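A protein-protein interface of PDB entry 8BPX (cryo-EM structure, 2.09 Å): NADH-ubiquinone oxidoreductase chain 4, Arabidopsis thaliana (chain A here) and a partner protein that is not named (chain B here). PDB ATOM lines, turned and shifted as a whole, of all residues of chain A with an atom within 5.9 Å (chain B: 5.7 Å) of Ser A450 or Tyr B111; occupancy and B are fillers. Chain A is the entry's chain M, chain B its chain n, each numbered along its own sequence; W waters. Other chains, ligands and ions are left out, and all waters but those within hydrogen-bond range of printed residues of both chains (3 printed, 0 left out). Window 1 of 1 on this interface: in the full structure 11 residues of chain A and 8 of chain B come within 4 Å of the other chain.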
ATOM      1  N   ASP A 357     -12.948  -9.004  -6.251  1.00  0.00           N
ATOM      2  CA  ASP A 357     -13.300  -9.740  -7.461  1.00  0.00           C
ATOM      3  C   ASP A 357     -12.159 -10.631  -7.935  1.00  0.00           C
ATOM      4  O   ASP A 357     -12.405 -11.705  -8.492  1.00  0.00           O
ATOM      5  CB  ASP A 357     -13.700  -8.771  -8.571  1.00  0.00           C
ATOM      6  CG  ASP A 357     -14.991  -8.038  -8.273  1.00  0.00           C
ATOM      7  OD1 ASP A 357     -15.559  -8.238  -7.179  1.00  0.00           O
ATOM      8  OD2 ASP A 357     -15.437  -7.254  -9.133  1.00  0.00           O
ATOM      9  N   ARG A 358     -10.912 -10.211  -7.719  1.00  0.00           N
ATOM     10  CA  ARG A 358      -9.765 -10.999  -8.154  1.00  0.00           C
ATOM     11  C   ARG A 358      -9.383 -12.059  -7.125  1.00  0.00           C
ATOM     12  O   ARG A 358      -9.141 -13.217  -7.479  1.00  0.00           O
ATOM     13  CB  ARG A 358      -8.572 -10.081  -8.431  1.00  0.00           C
ATOM     14  CG  ARG A 358      -8.821  -9.068  -9.530  1.00  0.00           C
ATOM     15  CD  ARG A 358      -7.957  -7.828  -9.361  1.00  0.00           C
ATOM     16  NE  ARG A 358      -7.802  -7.097 -10.611  1.00  0.00           N
ATOM     17  CZ  ARG A 358      -8.758  -6.384 -11.189  1.00  0.00           C
ATOM     18  NH1 ARG A 358      -9.956  -6.259 -10.642  1.00  0.00           N
ATOM     19  NH2 ARG A 358      -8.505  -5.778 -12.342  1.00  0.00           N
ATOM     20  N   HIS A 359      -9.265 -11.644  -5.873  1.00  0.00           N
ATOM     21  CA  HIS A 359      -8.663 -12.450  -4.793  1.00  0.00           C
ATOM     22  C   HIS A 359      -9.640 -13.094  -3.818  1.00  0.00           C
ATOM     23  O   HIS A 359      -9.174 -13.915  -3.102  1.00  0.00           O
ATOM     24  CB  HIS A 359      -7.535 -11.588  -4.143  1.00  0.00           C
ATOM     25  CG  HIS A 359      -6.615 -11.038  -5.172  1.00  0.00           C
ATOM     26  ND1 HIS A 359      -5.962 -11.844  -6.064  1.00  0.00           N
ATOM     27  CD2 HIS A 359      -6.271  -9.774  -5.483  1.00  0.00           C
ATOM     28  CE1 HIS A 359      -5.231 -11.114  -6.861  1.00  0.00           C
ATOM     29  NE2 HIS A 359      -5.397  -9.849  -6.525  1.00  0.00           N
ATOM     30  N   THR A 373       2.672  -4.595  -7.964  1.00  0.00           N
ATOM     31  CA  THR A 373       1.951  -5.316  -9.003  1.00  0.00           C
ATOM     32  C   THR A 373       0.753  -4.559  -9.556  1.00  0.00           C
ATOM     33  O   THR A 373       0.358  -4.824 -10.692  1.00  0.00           O
ATOM     34  CB  THR A 373       1.473  -6.693  -8.504  1.00  0.00           C
ATOM     35  OG1 THR A 373       0.634  -6.548  -7.351  1.00  0.00           O
ATOM     36  CG2 THR A 373       2.660  -7.583  -8.161  1.00  0.00           C
ATOM     37  N   MET A 374       0.172  -3.631  -8.796  1.00  0.00           N
ATOM     38  CA  MET A 374      -0.996  -2.863  -9.239  1.00  0.00           C
ATOM     39  C   MET A 374      -0.788  -1.373  -8.981  1.00  0.00           C
ATOM     40  O   MET A 374      -1.528  -0.754  -8.213  1.00  0.00           O
ATOM     41  CB  MET A 374      -2.260  -3.365  -8.542  1.00  0.00           C
ATOM     42  CG  MET A 374      -2.426  -4.881  -8.507  1.00  0.00           C
ATOM     43  SD  MET A 374      -3.808  -5.448  -7.488  1.00  0.00           S
ATOM     44  CE  MET A 374      -5.208  -4.660  -8.273  1.00  0.00           C
ATOM     45  N   LYS A 448      -0.533 -14.149  -8.131  1.00  0.00           N
ATOM     46  CA  LYS A 448      -1.046 -13.759  -9.458  1.00  0.00           C
ATOM     47  C   LYS A 448      -1.850 -12.448  -9.352  1.00  0.00           C
ATOM     48  O   LYS A 448      -2.708 -12.360  -8.555  1.00  0.00           O
ATOM     49  CB  LYS A 448      -1.707 -14.974 -10.108  1.00  0.00           C
ATOM     50  CG  LYS A 448      -2.410 -14.789 -11.427  1.00  0.00           C
ATOM     51  CD  LYS A 448      -3.010 -16.094 -11.908  1.00  0.00           C
ATOM     52  CE  LYS A 448      -1.962 -17.148 -12.169  1.00  0.00           C
ATOM     53  NZ  LYS A 448      -1.237 -16.869 -13.430  1.00  0.00           N
ATOM     54  N   PHE A 449      -1.551 -11.499 -10.217  1.00  0.00           N
ATOM     55  CA  PHE A 449      -2.117 -10.135 -10.089  1.00  0.00           C
ATOM     56  C   PHE A 449      -2.499  -9.546 -11.441  1.00  0.00           C
ATOM     57  O   PHE A 449      -1.985  -9.897 -12.444  1.00  0.00           O
ATOM     58  CB  PHE A 449      -1.204  -9.196  -9.248  1.00  0.00           C
ATOM     59  CG  PHE A 449      -0.728  -9.714  -7.926  1.00  0.00           C
ATOM     60  CD1 PHE A 449       0.402 -10.506  -7.846  1.00  0.00           C
ATOM     61  CD2 PHE A 449      -1.398  -9.379  -6.763  1.00  0.00           C
ATOM     62  CE1 PHE A 449       0.836 -10.980  -6.622  1.00  0.00           C
ATOM     63  CE2 PHE A 449      -0.955  -9.851  -5.544  1.00  0.00           C
ATOM     64  CZ  PHE A 449       0.157 -10.648  -5.476  1.00  0.00           C
ATOM     65  N   SER A 450      -3.434  -8.628 -11.396  1.00  0.00           N
ATOM     66  CA  SER A 450      -3.836  -7.857 -12.564  1.00  0.00           C
ATOM     67  C   SER A 450      -4.226  -6.461 -12.112  1.00  0.00           C
ATOM     68  O   SER A 450      -5.057  -6.312 -11.212  1.00  0.00           O
ATOM     69  CB  SER A 450      -5.007  -8.520 -13.295  1.00  0.00           C
ATOM     70  OG  SER A 450      -5.146  -7.994 -14.596  1.00  0.00           O
ATOM     71  N   ASP A 451      -3.633  -5.446 -12.736  1.00  0.00           N
ATOM     72  CA  ASP A 451      -4.039  -4.072 -12.486  1.00  0.00           C
ATOM     73  C   ASP A 451      -5.397  -3.809 -13.138  1.00  0.00           C
ATOM     74  O   ASP A 451      -6.018  -4.693 -13.729  1.00  0.00           O
ATOM     75  CB  ASP A 451      -2.973  -3.098 -12.992  1.00  0.00           C
ATOM     76  CG  ASP A 451      -2.792  -1.887 -12.073  1.00  0.00           C
ATOM     77  OD1 ASP A 451      -3.693  -1.591 -11.267  1.00  0.00           O
ATOM     78  OD2 ASP A 451      -1.745  -1.223 -12.168  1.00  0.00           O
ATOM     79  N   LEU A 452      -5.861  -2.569 -13.031  1.00  0.00           N
ATOM     80  CA  LEU A 452      -7.190  -2.221 -13.513  1.00  0.00           C
ATOM     81  C   LEU A 452      -7.292  -2.349 -15.029  1.00  0.00           C
ATOM     82  O   LEU A 452      -6.370  -1.990 -15.763  1.00  0.00           O
ATOM     83  CB  LEU A 452      -7.550  -0.801 -13.086  1.00  0.00           C
ATOM     84  CG  LEU A 452      -7.183  -0.419 -11.651  1.00  0.00           C
ATOM     85  CD1 LEU A 452      -7.184   1.086 -11.493  1.00  0.00           C
ATOM     86  CD2 LEU A 452      -8.130  -1.073 -10.653  1.00  0.00           C
ATOM     87  N   ASN A 453      -8.427  -2.869 -15.494  1.00  0.00           N
ATOM     88  CA  ASN A 453      -8.728  -2.858 -16.914  1.00  0.00           C
ATOM     89  C   ASN A 453      -9.368  -1.521 -17.292  1.00  0.00           C
ATOM     90  O   ASN A 453      -9.570  -0.639 -16.454  1.00  0.00           O
ATOM     91  CB  ASN A 453      -9.634  -4.033 -17.298  1.00  0.00           C
ATOM     92  CG  ASN A 453     -10.859  -4.160 -16.412  1.00  0.00           C
ATOM     93  OD1 ASN A 453     -11.592  -3.199 -16.197  1.00  0.00           O
ATOM     94  ND2 ASN A 453     -11.100  -5.361 -15.917  1.00  0.00           N
ATOM     95  N   ARG A 455     -12.431  -0.711 -18.163  1.00  0.00           N
ATOM     96  CA  ARG A 455     -13.715  -0.426 -17.528  1.00  0.00           C
ATOM     97  C   ARG A 455     -13.528   0.145 -16.127  1.00  0.00           C
ATOM     98  O   ARG A 455     -14.196   1.112 -15.750  1.00  0.00           O
ATOM     99  CB  ARG A 455     -14.574  -1.690 -17.485  1.00  0.00           C
ATOM    100  CG  ARG A 455     -16.060  -1.435 -17.256  1.00  0.00           C
ATOM    101  CD  ARG A 455     -16.889  -2.708 -17.397  1.00  0.00           C
ATOM    102  NE  ARG A 455     -16.096  -3.892 -17.097  1.00  0.00           N
ATOM    103  CZ  ARG A 455     -15.920  -4.391 -15.883  1.00  0.00           C
ATOM    104  NH1 ARG A 455     -16.529  -3.876 -14.828  1.00  0.00           N
ATOM    105  NH2 ARG A 455     -15.104  -5.425 -15.720  1.00  0.00           N
ATOM    106  N   GLU A 456     -12.621  -0.442 -15.347  1.00  0.00           N
ATOM    107  CA  GLU A 456     -12.393   0.017 -13.981  1.00  0.00           C
ATOM    108  C   GLU A 456     -11.801   1.425 -13.953  1.00  0.00           C
ATOM    109  O   GLU A 456     -12.218   2.268 -13.145  1.00  0.00           O
ATOM    110  CB  GLU A 456     -11.499  -0.991 -13.257  1.00  0.00           C
ATOM    111  CG  GLU A 456     -12.244  -2.253 -12.817  1.00  0.00           C
ATOM    112  CD  GLU A 456     -11.329  -3.430 -12.505  1.00  0.00           C
ATOM    113  OE1 GLU A 456     -10.112  -3.346 -12.755  1.00  0.00           O
ATOM    114  OE2 GLU A 456     -11.829  -4.440 -11.981  1.00  0.00           O
ATOM    115  N   ILE B 107       1.809 -11.922 -13.754  1.00  0.00           N
ATOM    116  CA  ILE B 107       0.956 -10.783 -14.067  1.00  0.00           C
ATOM    117  C   ILE B 107      -0.018 -11.220 -15.149  1.00  0.00           C
ATOM    118  O   ILE B 107       0.397 -11.763 -16.179  1.00  0.00           O
ATOM    119  CB  ILE B 107       1.788  -9.573 -14.531  1.00  0.00           C
ATOM    120  CG1 ILE B 107       2.771  -9.125 -13.442  1.00  0.00           C
ATOM    121  CG2 ILE B 107       0.885  -8.427 -14.940  1.00  0.00           C
ATOM    122  CD1 ILE B 107       2.153  -8.838 -12.101  1.00  0.00           C
ATOM    123  N   VAL B 108      -1.295 -11.009 -14.946  1.00  0.00           N
ATOM    124  CA  VAL B 108      -2.333 -11.496 -15.905  1.00  0.00           C
ATOM    125  C   VAL B 108      -2.780 -10.324 -16.765  1.00  0.00           C
ATOM    126  O   VAL B 108      -2.967  -9.215 -16.263  1.00  0.00           O
ATOM    127  CB  VAL B 108      -3.559 -12.173 -15.230  1.00  0.00           C
ATOM    128  CG1 VAL B 108      -4.572 -12.770 -16.175  1.00  0.00           C
ATOM    129  CG2 VAL B 108      -3.217 -13.084 -14.083  1.00  0.00           C
ATOM    130  N   TYR B 109      -2.988 -10.605 -18.003  1.00  0.00           N
ATOM    131  CA  TYR B 109      -3.449  -9.657 -19.002  1.00  0.00           C
ATOM    132  C   TYR B 109      -4.875 -10.001 -19.410  1.00  0.00           C
ATOM    133  O   TYR B 109      -5.312 -11.147 -19.280  1.00  0.00           O
ATOM    134  CB  TYR B 109      -2.532  -9.676 -20.227  1.00  0.00           C
ATOM    135  CG  TYR B 109      -1.183  -9.045 -19.987  1.00  0.00           C
ATOM    136  CD1 TYR B 109      -1.015  -8.057 -19.028  1.00  0.00           C
ATOM    137  CD2 TYR B 109      -0.067  -9.474 -20.688  1.00  0.00           C
ATOM    138  CE1 TYR B 109       0.221  -7.488 -18.803  1.00  0.00           C
ATOM    139  CE2 TYR B 109       1.168  -8.919 -20.470  1.00  0.00           C
ATOM    140  CZ  TYR B 109       1.309  -7.927 -19.526  1.00  0.00           C
ATOM    141  OH  TYR B 109       2.546  -7.375 -19.311  1.00  0.00           O
ATOM    142  N   ASN B 110      -5.599  -8.987 -19.886  1.00  0.00           N
ATOM    143  CA  ASN B 110      -6.947  -9.149 -20.434  1.00  0.00           C
ATOM    144  C   ASN B 110      -7.915  -9.739 -19.407  1.00  0.00           C
ATOM    145  O   ASN B 110      -8.713 -10.629 -19.704  1.00  0.00           O
ATOM    146  CB  ASN B 110      -6.917  -9.995 -21.712  1.00  0.00           C
ATOM    147  CG  ASN B 110      -5.825  -9.560 -22.667  1.00  0.00           C
ATOM    148  OD1 ASN B 110      -5.745  -8.394 -23.045  1.00  0.00           O
ATOM    149  ND2 ASN B 110      -4.974 -10.493 -23.054  1.00  0.00           N
ATOM    150  N   TYR B 111      -7.847  -9.222 -18.189  1.00  0.00           N
ATOM    151  CA  TYR B 111      -8.759  -9.608 -17.127  1.00  0.00           C
ATOM    152  C   TYR B 111     -10.064  -8.822 -17.217  1.00  0.00           C
ATOM    153  O   TYR B 111     -10.096  -7.679 -17.676  1.00  0.00           O
ATOM    154  CB  TYR B 111      -8.112  -9.384 -15.760  1.00  0.00           C
ATOM    155  CG  TYR B 111      -8.975  -9.804 -14.593  1.00  0.00           C
ATOM    156  CD1 TYR B 111      -9.134 -11.144 -14.267  1.00  0.00           C
ATOM    157  CD2 TYR B 111      -9.642  -8.859 -13.826  1.00  0.00           C
ATOM    158  CE1 TYR B 111      -9.925 -11.530 -13.209  1.00  0.00           C
ATOM    159  CE2 TYR B 111     -10.435  -9.235 -12.769  1.00  0.00           C
ATOM    160  CZ  TYR B 111     -10.573 -10.575 -12.462  1.00  0.00           C
ATOM    161  OH  TYR B 111     -11.366 -10.959 -11.407  1.00  0.00           O
ATOM    162  N   GLY B 112     -11.145  -9.458 -16.778  1.00  0.00           N
ATOM    163  CA  GLY B 112     -12.430  -8.794 -16.657  1.00  0.00           C
ATOM    164  C   GLY B 112     -13.076  -8.353 -17.953  1.00  0.00           C
ATOM    165  O   GLY B 112     -13.773  -7.337 -17.967  1.00  0.00           O
ATOM    166  N   LEU B 113     -12.869  -9.090 -19.039  1.00  0.00           N
ATOM    167  CA  LEU B 113     -13.496  -8.754 -20.308  1.00  0.00           C
ATOM    168  C   LEU B 113     -14.993  -9.047 -20.262  1.00  0.00           C
ATOM    169  O   LEU B 113     -15.457  -9.898 -19.502  1.00  0.00           O
ATOM    170  CB  LEU B 113     -12.839  -9.536 -21.445  1.00  0.00           C
ATOM    171  CG  LEU B 113     -11.340  -9.263 -21.598  1.00  0.00           C
ATOM    172  CD1 LEU B 113     -10.688 -10.238 -22.556  1.00  0.00           C
ATOM    173  CD2 LEU B 113     -11.124  -7.838 -22.057  1.00  0.00           C
HETATM  174  O   HOH W   1     -10.072 -13.416 -10.369  1.00  0.00           O
HETATM  175  O   HOH W   2     -15.075  -5.282 -19.193  1.00  0.00           O
HETATM  176  O   HOH W   3      -0.863 -14.251 -15.576  1.00  0.00           O
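The backbone carbonyl oxygen (O) of Phe A449 is in hydrogen-bond range of the backbone NH (N) of Val B108. The side-chain amide nitrogen (ND2) of Asn A453 lies within hydrogen-bond range of the backbone carbonyl oxygen (O) of Tyr B111. The side-chain hydroxyl (OH) of Tyr B111 sits at hydrogen-bond distance from the backbone carbonyl oxygen (O) of Asp A357 (3.2 Å). The backbone carbonyl oxygen of Val B108 is in hydrogen-bond range of the side-chain hydroxyl of Ser A450 (3.0 Å). The backbone carbonyl oxygen (O) of Gly B112 lies within hydrogen-bond range of the guanidinium group (NH2) of Arg A455, 3.2 Å away.
Printed residues of chain B within 4 Å of Asp A357: Tyr B111. Of the printed residues of chain B, Arg A358 touches Tyr B111. Ser A450 touches just these residues of chain B: Val B108 and Tyr B111. Tyr B111 touches just these residues of chain A: Asp A357, Arg A358, Ser A450 and Asn A453. The nearest residue of chain B that does not touch Ser A450 is Tyr B109 (4.8 Å). The nearest residue of chain A that does not touch Tyr B111 is Glu A456 (5.1 Å).
The guanidinium group (NH1) of Arg A358 is in salt-bridge range of the side-chain carboxylate (OE2) of Glu A456, at 2.9 Å. The backbone carbonyl oxygen of Asp A451 is in hydrogen-bond range of the guanidinium group of Arg A358, 3.0 Å away. The guanidinium group (NE) of Arg A358 sits at hydrogen-bond distance from the backbone carbonyl oxygen (O) of Ser A450, at 2.9 Å. N of Glu A456 sits at hydrogen-bond distance from OD1 of Asn A453. The side-chain amide oxygen (OD1) of Asn A453 sits at hydrogen-bond distance from the backbone NH (N) of Arg A455, at 3.3 Å.
Arg A358 touches Tyr B111. Val B108 touches Lys A448. Phe A449 touches Ile B107. Ser A450 touches Tyr B111. Asn A453 touches Gly B112 (ND2 to CA, 3.8 Å).
Water W2 bridges the guanidinium group (NE) of Arg A455 (2.7 Å) and the backbone carbonyl oxygen (O) of Gly B112 (2.7 Å). Water W3 lies within hydrogen-bond range of the backbone carbonyl oxygen of Ile B107, the backbone NH of Val B108 and the side-chain amino group of Lys A448. Water W1 lies within hydrogen-bond range of OH of Tyr B111 (3.0 Å), O of Arg A358 (3.0 Å) and O of Asp A357 (3.4 Å).
Hydrophobic or aromatic side chains of chain B within 4 Å of the printed part of chain A: Val B108 and Tyr B111. Among the printed residues, 10 pairs touch across the chains.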
